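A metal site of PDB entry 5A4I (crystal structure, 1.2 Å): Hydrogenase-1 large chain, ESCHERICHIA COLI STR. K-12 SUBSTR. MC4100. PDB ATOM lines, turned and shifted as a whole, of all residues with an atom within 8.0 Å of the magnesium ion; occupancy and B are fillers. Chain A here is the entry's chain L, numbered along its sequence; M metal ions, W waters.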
ATOM      1  N   PHE A  53     -20.174 -28.235  -2.498  1.00  0.00           N
ATOM      2  CA  PHE A  53     -19.883 -27.434  -3.678  1.00  0.00           C
ATOM      3  C   PHE A  53     -19.522 -28.391  -4.803  1.00  0.00           C
ATOM      4  O   PHE A  53     -18.819 -29.360  -4.567  1.00  0.00           O
ATOM      5  CB  PHE A  53     -18.712 -26.465  -3.414  1.00  0.00           C
ATOM      6  CG  PHE A  53     -18.265 -25.692  -4.646  1.00  0.00           C
ATOM      7  CD1 PHE A  53     -18.973 -24.613  -5.128  1.00  0.00           C
ATOM      8  CD2 PHE A  53     -17.108 -26.058  -5.317  1.00  0.00           C
ATOM      9  CE1 PHE A  53     -18.549 -23.910  -6.244  1.00  0.00           C
ATOM     10  CE2 PHE A  53     -16.719 -25.352  -6.449  1.00  0.00           C
ATOM     11  CZ  PHE A  53     -17.398 -24.262  -6.873  1.00  0.00           C
ATOM     12  N   GLU A  57     -20.431 -23.481 -12.446  1.00  0.00           N
ATOM     13  CA  GLU A  57     -19.994 -22.292 -13.189  1.00  0.00           C
ATOM     14  C   GLU A  57     -18.634 -22.450 -13.870  1.00  0.00           C
ATOM     15  O   GLU A  57     -18.373 -21.825 -14.901  1.00  0.00           O
ATOM     16  CB  GLU A  57     -19.975 -21.080 -12.270  1.00  0.00           C
ATOM     17  CG  GLU A  57     -21.371 -20.722 -11.720  1.00  0.00           C
ATOM     18  CD  GLU A  57     -21.362 -19.975 -10.419  1.00  0.00           C
ATOM     19  OE1 GLU A  57     -20.413 -20.184  -9.607  1.00  0.00           O
ATOM     20  OE2 GLU A  57     -22.340 -19.234 -10.148  1.00  0.00           O
ATOM     21  N   ILE A  75     -27.930 -28.658 -11.614  1.00  0.00           N
ATOM     22  CA  ILE A  75     -27.746 -27.965 -10.340  1.00  0.00           C
ATOM     23  C   ILE A  75     -28.658 -28.589  -9.323  1.00  0.00           C
ATOM     24  O   ILE A  75     -28.273 -28.704  -8.156  1.00  0.00           O
ATOM     25  CB  ILE A  75     -27.981 -26.447 -10.489  1.00  0.00           C
ATOM     26  CG1 ILE A  75     -26.776 -25.822 -11.218  1.00  0.00           C
ATOM     27  CG2 ILE A  75     -28.149 -25.814  -9.127  1.00  0.00           C
ATOM     28  CD1 ILE A  75     -26.988 -24.392 -11.622  1.00  0.00           C
ATOM     29  N   GLU A 347     -22.373 -10.120  -5.453  1.00  0.00           N
ATOM     30  CA  GLU A 347     -22.084 -11.188  -4.522  1.00  0.00           C
ATOM     31  C   GLU A 347     -20.736 -10.945  -3.841  1.00  0.00           C
ATOM     32  O   GLU A 347     -19.728 -10.613  -4.483  1.00  0.00           O
ATOM     33  CB  GLU A 347     -22.037 -12.556  -5.222  1.00  0.00           C
ATOM     34  CG  GLU A 347     -23.375 -13.017  -5.745  1.00  0.00           C
ATOM     35  CD  GLU A 347     -23.273 -14.368  -6.394  1.00  0.00           C
ATOM     36  OE1 GLU A 347     -22.638 -14.458  -7.454  1.00  0.00           O
ATOM     37  OE2 GLU A 347     -23.856 -15.322  -5.803  1.00  0.00           O
ATOM     38  N   TYR A 354     -14.161 -18.775  -1.120  1.00  0.00           N
ATOM     39  CA  TYR A 354     -13.817 -18.393  -2.460  1.00  0.00           C
ATOM     40  C   TYR A 354     -12.765 -17.289  -2.437  1.00  0.00           C
ATOM     41  O   TYR A 354     -12.646 -16.555  -1.457  1.00  0.00           O
ATOM     42  CB  TYR A 354     -15.040 -17.822  -3.202  1.00  0.00           C
ATOM     43  CG  TYR A 354     -16.173 -18.808  -3.362  1.00  0.00           C
ATOM     44  CD1 TYR A 354     -16.132 -19.748  -4.362  1.00  0.00           C
ATOM     45  CD2 TYR A 354     -17.216 -18.884  -2.472  1.00  0.00           C
ATOM     46  CE1 TYR A 354     -17.088 -20.712  -4.456  1.00  0.00           C
ATOM     47  CE2 TYR A 354     -18.199 -19.815  -2.559  1.00  0.00           C
ATOM     48  CZ  TYR A 354     -18.128 -20.758  -3.561  1.00  0.00           C
ATOM     49  OH  TYR A 354     -19.101 -21.728  -3.692  1.00  0.00           O
ATOM     50  N   PRO A 365     -22.780 -10.392 -11.263  1.00  0.00           N
ATOM     51  CA  PRO A 365     -22.415 -11.695 -11.893  1.00  0.00           C
ATOM     52  C   PRO A 365     -21.724 -11.654 -13.239  1.00  0.00           C
ATOM     53  O   PRO A 365     -20.980 -12.584 -13.546  1.00  0.00           O
ATOM     54  CB  PRO A 365     -23.781 -12.401 -11.997  1.00  0.00           C
ATOM     55  CG  PRO A 365     -24.551 -11.841 -10.822  1.00  0.00           C
ATOM     56  CD  PRO A 365     -24.178 -10.389 -10.807  1.00  0.00           C
ATOM     57  N   GLY A 368     -18.421 -11.928 -12.212  1.00  0.00           N
ATOM     58  CA  GLY A 368     -18.299 -12.914 -11.179  1.00  0.00           C
ATOM     59  C   GLY A 368     -17.070 -13.792 -11.303  1.00  0.00           C
ATOM     60  O   GLY A 368     -16.502 -13.952 -12.392  1.00  0.00           O
ATOM     61  N   ILE A 369     -16.676 -14.340 -10.165  1.00  0.00           N
ATOM     62  CA  ILE A 369     -15.506 -15.198 -10.078  1.00  0.00           C
ATOM     63  C   ILE A 369     -15.887 -16.352  -9.184  1.00  0.00           C
ATOM     64  O   ILE A 369     -16.362 -16.146  -8.079  1.00  0.00           O
ATOM     65  CB  ILE A 369     -14.257 -14.492  -9.519  1.00  0.00           C
ATOM     66  CG1 ILE A 369     -13.884 -13.234 -10.311  1.00  0.00           C
ATOM     67  CG2 ILE A 369     -13.079 -15.456  -9.425  1.00  0.00           C
ATOM     68  CD1 ILE A 369     -12.846 -12.371  -9.646  1.00  0.00           C
ATOM     69  N   THR A 370     -15.580 -17.570  -9.639  1.00  0.00           N
ATOM     70  CA  THR A 370     -15.799 -18.758  -8.828  1.00  0.00           C
ATOM     71  C   THR A 370     -14.499 -19.554  -8.740  1.00  0.00           C
ATOM     72  O   THR A 370     -14.215 -20.409  -9.579  1.00  0.00           O
ATOM     73  CB  THR A 370     -16.957 -19.613  -9.378  1.00  0.00           C
ATOM     74  OG1 THR A 370     -18.100 -18.764  -9.455  1.00  0.00           O
ATOM     75  CG2 THR A 370     -17.229 -20.839  -8.463  1.00  0.00           C
ATOM     76  N   TRP A 397     -19.793 -22.533   1.766  1.00  0.00           N
ATOM     77  CA  TRP A 397     -19.658 -22.626   0.305  1.00  0.00           C
ATOM     78  C   TRP A 397     -20.676 -21.764  -0.437  1.00  0.00           C
ATOM     79  O   TRP A 397     -20.706 -21.760  -1.665  1.00  0.00           O
ATOM     80  CB  TRP A 397     -19.773 -24.080  -0.171  1.00  0.00           C
ATOM     81  CG  TRP A 397     -18.561 -24.932   0.162  1.00  0.00           C
ATOM     82  CD1 TRP A 397     -18.487 -25.948   1.047  1.00  0.00           C
ATOM     83  CD2 TRP A 397     -17.240 -24.755  -0.397  1.00  0.00           C
ATOM     84  NE1 TRP A 397     -17.205 -26.479   1.033  1.00  0.00           N
ATOM     85  CE2 TRP A 397     -16.424 -25.746   0.192  1.00  0.00           C
ATOM     86  CE3 TRP A 397     -16.698 -23.918  -1.363  1.00  0.00           C
ATOM     87  CZ2 TRP A 397     -15.057 -25.864  -0.098  1.00  0.00           C
ATOM     88  CZ3 TRP A 397     -15.346 -24.022  -1.643  1.00  0.00           C
ATOM     89  CH2 TRP A 397     -14.558 -24.978  -1.024  1.00  0.00           C
ATOM     90  N   ILE A 398     -21.503 -21.023   0.290  1.00  0.00           N
ATOM     91  CA  ILE A 398     -22.513 -20.199  -0.364  1.00  0.00           C
ATOM     92  C   ILE A 398     -21.974 -18.752  -0.428  1.00  0.00           C
ATOM     93  O   ILE A 398     -21.557 -18.196   0.591  1.00  0.00           O
ATOM     94  CB  ILE A 398     -23.835 -20.221   0.442  1.00  0.00           C
ATOM     95  CG1 ILE A 398     -24.284 -21.644   0.716  1.00  0.00           C
ATOM     96  CG2 ILE A 398     -24.933 -19.400  -0.242  1.00  0.00           C
ATOM     97  CD1 ILE A 398     -25.483 -21.742   1.623  1.00  0.00           C
ATOM     98  N   LYS A 399     -21.977 -18.147  -1.622  1.00  0.00           N
ATOM     99  CA  LYS A 399     -21.674 -16.720  -1.773  1.00  0.00           C
ATOM    100  C   LYS A 399     -22.757 -15.884  -1.101  1.00  0.00           C
ATOM    101  O   LYS A 399     -23.863 -16.345  -0.837  1.00  0.00           O
ATOM    102  CB  LYS A 399     -21.527 -16.342  -3.216  1.00  0.00           C
ATOM    103  CG  LYS A 399     -20.402 -17.022  -3.981  1.00  0.00           C
ATOM    104  CD  LYS A 399     -20.260 -16.459  -5.391  1.00  0.00           C
ATOM    105  CE  LYS A 399     -19.137 -17.105  -6.197  1.00  0.00           C
ATOM    106  NZ  LYS A 399     -19.276 -16.722  -7.643  1.00  0.00           N
ATOM    107  N   PRO A 401     -25.119 -12.880  -1.768  1.00  0.00           N
ATOM    108  CA  PRO A 401     -25.731 -11.896  -2.685  1.00  0.00           C
ATOM    109  C   PRO A 401     -26.375 -10.762  -1.908  1.00  0.00           C
ATOM    110  O   PRO A 401     -26.942 -11.000  -0.829  1.00  0.00           O
ATOM    111  CB  PRO A 401     -26.765 -12.701  -3.490  1.00  0.00           C
ATOM    112  CG  PRO A 401     -26.562 -14.125  -3.054  1.00  0.00           C
ATOM    113  CD  PRO A 401     -25.986 -14.061  -1.654  1.00  0.00           C
ATOM    114  N   GLY A 513     -31.376 -16.161 -11.205  1.00  0.00           N
ATOM    115  CA  GLY A 513     -30.778 -15.548 -12.402  1.00  0.00           C
ATOM    116  C   GLY A 513     -29.585 -16.378 -12.882  1.00  0.00           C
ATOM    117  O   GLY A 513     -28.804 -16.888 -12.049  1.00  0.00           O
ATOM    118  N   TRP A 515     -26.437 -15.555 -15.617  1.00  0.00           N
ATOM    119  CA  TRP A 515     -25.741 -14.565 -16.423  1.00  0.00           C
ATOM    120  C   TRP A 515     -24.746 -15.287 -17.289  1.00  0.00           C
ATOM    121  O   TRP A 515     -23.865 -16.007 -16.765  1.00  0.00           O
ATOM    122  CB  TRP A 515     -25.087 -13.522 -15.506  1.00  0.00           C
ATOM    123  CG  TRP A 515     -25.948 -12.592 -14.798  1.00  0.00           C
ATOM    124  CD1 TRP A 515     -26.108 -11.300 -15.136  1.00  0.00           C
ATOM    125  CD2 TRP A 515     -26.753 -12.790 -13.604  1.00  0.00           C
ATOM    126  NE1 TRP A 515     -26.985 -10.660 -14.251  1.00  0.00           N
ATOM    127  CE2 TRP A 515     -27.379 -11.556 -13.304  1.00  0.00           C
ATOM    128  CE3 TRP A 515     -27.025 -13.889 -12.763  1.00  0.00           C
ATOM    129  CZ2 TRP A 515     -28.185 -11.374 -12.202  1.00  0.00           C
ATOM    130  CZ3 TRP A 515     -27.841 -13.705 -11.670  1.00  0.00           C
ATOM    131  CH2 TRP A 515     -28.424 -12.445 -11.412  1.00  0.00           C
ATOM    132  N   TYR A 526     -20.288 -18.091 -17.050  1.00  0.00           N
ATOM    133  CA  TYR A 526     -21.630 -18.515 -16.695  1.00  0.00           C
ATOM    134  C   TYR A 526     -21.736 -18.427 -15.183  1.00  0.00           C
ATOM    135  O   TYR A 526     -21.092 -19.186 -14.512  1.00  0.00           O
ATOM    136  CB  TYR A 526     -21.881 -19.939 -17.185  1.00  0.00           C
ATOM    137  CG  TYR A 526     -23.371 -20.231 -17.373  1.00  0.00           C
ATOM    138  CD1 TYR A 526     -24.207 -20.344 -16.316  1.00  0.00           C
ATOM    139  CD2 TYR A 526     -23.924 -20.335 -18.659  1.00  0.00           C
ATOM    140  CE1 TYR A 526     -25.575 -20.592 -16.489  1.00  0.00           C
ATOM    141  CE2 TYR A 526     -25.267 -20.599 -18.833  1.00  0.00           C
ATOM    142  CZ  TYR A 526     -26.088 -20.701 -17.768  1.00  0.00           C
ATOM    143  OH  TYR A 526     -27.452 -20.944 -17.954  1.00  0.00           O
ATOM    144  N   GLN A 527     -22.498 -17.459 -14.717  1.00  0.00           N
ATOM    145  CA  GLN A 527     -22.649 -17.223 -13.297  1.00  0.00           C
ATOM    146  C   GLN A 527     -24.102 -17.312 -12.891  1.00  0.00           C
ATOM    147  O   GLN A 527     -24.989 -16.720 -13.506  1.00  0.00           O
ATOM    148  CB  GLN A 527     -22.058 -15.846 -12.878  1.00  0.00           C
ATOM    149  CG  GLN A 527     -20.530 -15.844 -12.950  1.00  0.00           C
ATOM    150  CD  GLN A 527     -19.891 -16.523 -11.766  1.00  0.00           C
ATOM    151  OE1 GLN A 527     -20.352 -16.426 -10.663  1.00  0.00           O
ATOM    152  NE2 GLN A 527     -18.800 -17.170 -11.997  1.00  0.00           N
ATOM    153  N   CYS A 528     -24.319 -18.050 -11.809  1.00  0.00           N
ATOM    154  CA  CYS A 528     -25.649 -18.289 -11.301  1.00  0.00           C
ATOM    155  C   CYS A 528     -25.813 -17.706  -9.903  1.00  0.00           C
ATOM    156  O   CYS A 528     -24.911 -17.845  -9.074  1.00  0.00           O
ATOM    157  CB  CYS A 528     -25.977 -19.773 -11.202  1.00  0.00           C
ATOM    158  SG  CYS A 528     -25.807 -20.691 -12.761  1.00  0.00           S
ATOM    159  N   VAL A 529     -26.932 -17.047  -9.659  1.00  0.00           N
ATOM    160  CA  VAL A 529     -27.303 -16.609  -8.306  1.00  0.00           C
ATOM    161  C   VAL A 529     -28.691 -17.183  -8.091  1.00  0.00           C
ATOM    162  O   VAL A 529     -29.616 -16.889  -8.864  1.00  0.00           O
ATOM    163  CB  VAL A 529     -27.291 -15.087  -8.138  1.00  0.00           C
ATOM    164  CG1 VAL A 529     -27.536 -14.770  -6.677  1.00  0.00           C
ATOM    165  CG2 VAL A 529     -25.989 -14.501  -8.640  1.00  0.00           C
ATOM    166  N   VAL A 530     -28.847 -18.041  -7.089  1.00  0.00           N
ATOM    167  CA  VAL A 530     -30.006 -18.923  -6.988  1.00  0.00           C
ATOM    168  C   VAL A 530     -30.764 -18.571  -5.698  1.00  0.00           C
ATOM    169  O   VAL A 530     -30.194 -17.946  -4.810  1.00  0.00           O
ATOM    170  CB  VAL A 530     -29.485 -20.378  -7.034  1.00  0.00           C
ATOM    171  CG1 VAL A 530     -30.541 -21.407  -7.076  1.00  0.00           C
ATOM    172  CG2 VAL A 530     -28.554 -20.573  -8.205  1.00  0.00           C
ATOM    173  N   THR A 533     -29.143 -19.298  -2.478  1.00  0.00           N
ATOM    174  CA  THR A 533     -27.961 -18.467  -2.274  1.00  0.00           C
ATOM    175  C   THR A 533     -28.309 -17.177  -1.505  1.00  0.00           C
ATOM    176  O   THR A 533     -27.597 -16.772  -0.608  1.00  0.00           O
ATOM    177  CB  THR A 533     -27.299 -18.113  -3.589  1.00  0.00           C
ATOM    178  OG1 THR A 533     -27.244 -19.194  -4.524  1.00  0.00           O
ATOM    179  CG2 THR A 533     -25.912 -17.567  -3.379  1.00  0.00           C
ATOM    180  N   CYS A 579     -28.788 -26.153  -5.006  1.00  0.00           N
ATOM    181  CA  CYS A 579     -29.057 -24.913  -5.678  1.00  0.00           C
ATOM    182  C   CYS A 579     -28.155 -23.789  -5.168  1.00  0.00           C
ATOM    183  O   CYS A 579     -27.640 -22.975  -5.947  1.00  0.00           O
ATOM    184  CB  CYS A 579     -30.525 -24.488  -5.493  1.00  0.00           C
ATOM    185  SG  CYS A 579     -31.592 -25.128  -6.746  1.00  0.00           S
ATOM    186  N   SER A 580     -28.040 -23.667  -3.839  1.00  0.00           N
ATOM    187  CA  SER A 580     -27.386 -22.498  -3.277  1.00  0.00           C
ATOM    188  C   SER A 580     -25.935 -22.394  -3.678  1.00  0.00           C
ATOM    189  O   SER A 580     -25.376 -21.275  -3.734  1.00  0.00           O
ATOM    190  CB  SER A 580     -27.517 -22.506  -1.762  1.00  0.00           C
ATOM    191  OG  SER A 580     -26.633 -23.427  -1.145  1.00  0.00           O
ATOM    192  N   THR A 581     -25.273 -23.550  -3.845  1.00  0.00           N
ATOM    193  CA  THR A 581     -23.847 -23.650  -4.067  1.00  0.00           C
ATOM    194  C   THR A 581     -23.439 -23.929  -5.505  1.00  0.00           C
ATOM    195  O   THR A 581     -22.438 -23.411  -5.982  1.00  0.00           O
ATOM    196  CB  THR A 581     -23.263 -24.726  -3.123  1.00  0.00           C
ATOM    197  OG1 THR A 581     -23.939 -25.963  -3.344  1.00  0.00           O
ATOM    198  CG2 THR A 581     -23.369 -24.297  -1.648  1.00  0.00           C
ATOM    199  N   HIS A 582     -24.224 -24.753  -6.196  1.00  0.00           N
ATOM    200  CA  HIS A 582     -23.992 -25.088  -7.581  1.00  0.00           C
ATOM    201  C   HIS A 582     -22.520 -25.368  -7.871  1.00  0.00           C
ATOM    202  O   HIS A 582     -22.021 -24.891  -8.896  1.00  0.00           O
ATOM    203  CB  HIS A 582     -24.689 -24.094  -8.530  1.00  0.00           C
ATOM    204  CG  HIS A 582     -24.533 -22.630  -8.171  1.00  0.00           C
ATOM    205  ND1 HIS A 582     -25.333 -22.018  -7.240  1.00  0.00           N
ATOM    206  CD2 HIS A 582     -23.717 -21.665  -8.632  1.00  0.00           C
ATOM    207  CE1 HIS A 582     -24.983 -20.749  -7.108  1.00  0.00           C
ATOM    208  NE2 HIS A 582     -24.011 -20.500  -7.947  1.00  0.00           N
ATOM    209  OXT HIS A 582     -21.874 -26.146  -7.099  1.00  0.00           O
HETATM  210 MG    MG M   1     -23.067 -18.527  -8.259  1.00  0.00          MG
HETATM  211  O   HOH W   1     -22.161 -16.711  -8.690  1.00  0.00           O
HETATM  212  O   HOH W   2     -21.265 -19.178  -7.357  1.00  0.00           O
HETATM  213  O   HOH W   3     -23.739 -17.888  -6.407  1.00  0.00           O
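The side-chain amide oxygen (OE1) of Gln 527 lies close to the side-chain carboxylate (OE2) of Glu 57 (3.5 Å).
The side-chain hydroxyl (OG1) of Thr 370 is in hydrogen-bond range of the side-chain carboxylate (OE1) of Glu 57.
The backbone carbonyl oxygen of Cys 579 is in hydrogen-bond range of a ring nitrogen (ND1) of His 582 (2.8 Å).
The nearest printed residue that does not touch the magnesium ion is Glu 347 (4.1 Å).
The magnesium ion is bound by water W3 (2.1 Å), water W1 (2.1 Å), water W2 (2.1 Å), the backbone carbonyl oxygen of Cys 528 (2.1 Å), the side-chain carboxylate of Glu 57 (2.1 Å) and a ring nitrogen (NE2) of His 582 (2.2 Å).
The magnesium ion has six donor atoms within binding distance.
Water W1 lies within hydrogen-bond range of the side-chain carboxylate (OE1) of Glu 347 (2.6 Å), the side-chain amide oxygen (OE1) of Gln 527 (2.7 Å) and the side-chain amino group (NZ) of Lys 399 (3.1 Å).
Water W2 lies within hydrogen-bond range of OE1 of Glu 57 (2.6 Å) and NZ of Lys 399 (3.2 Å).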
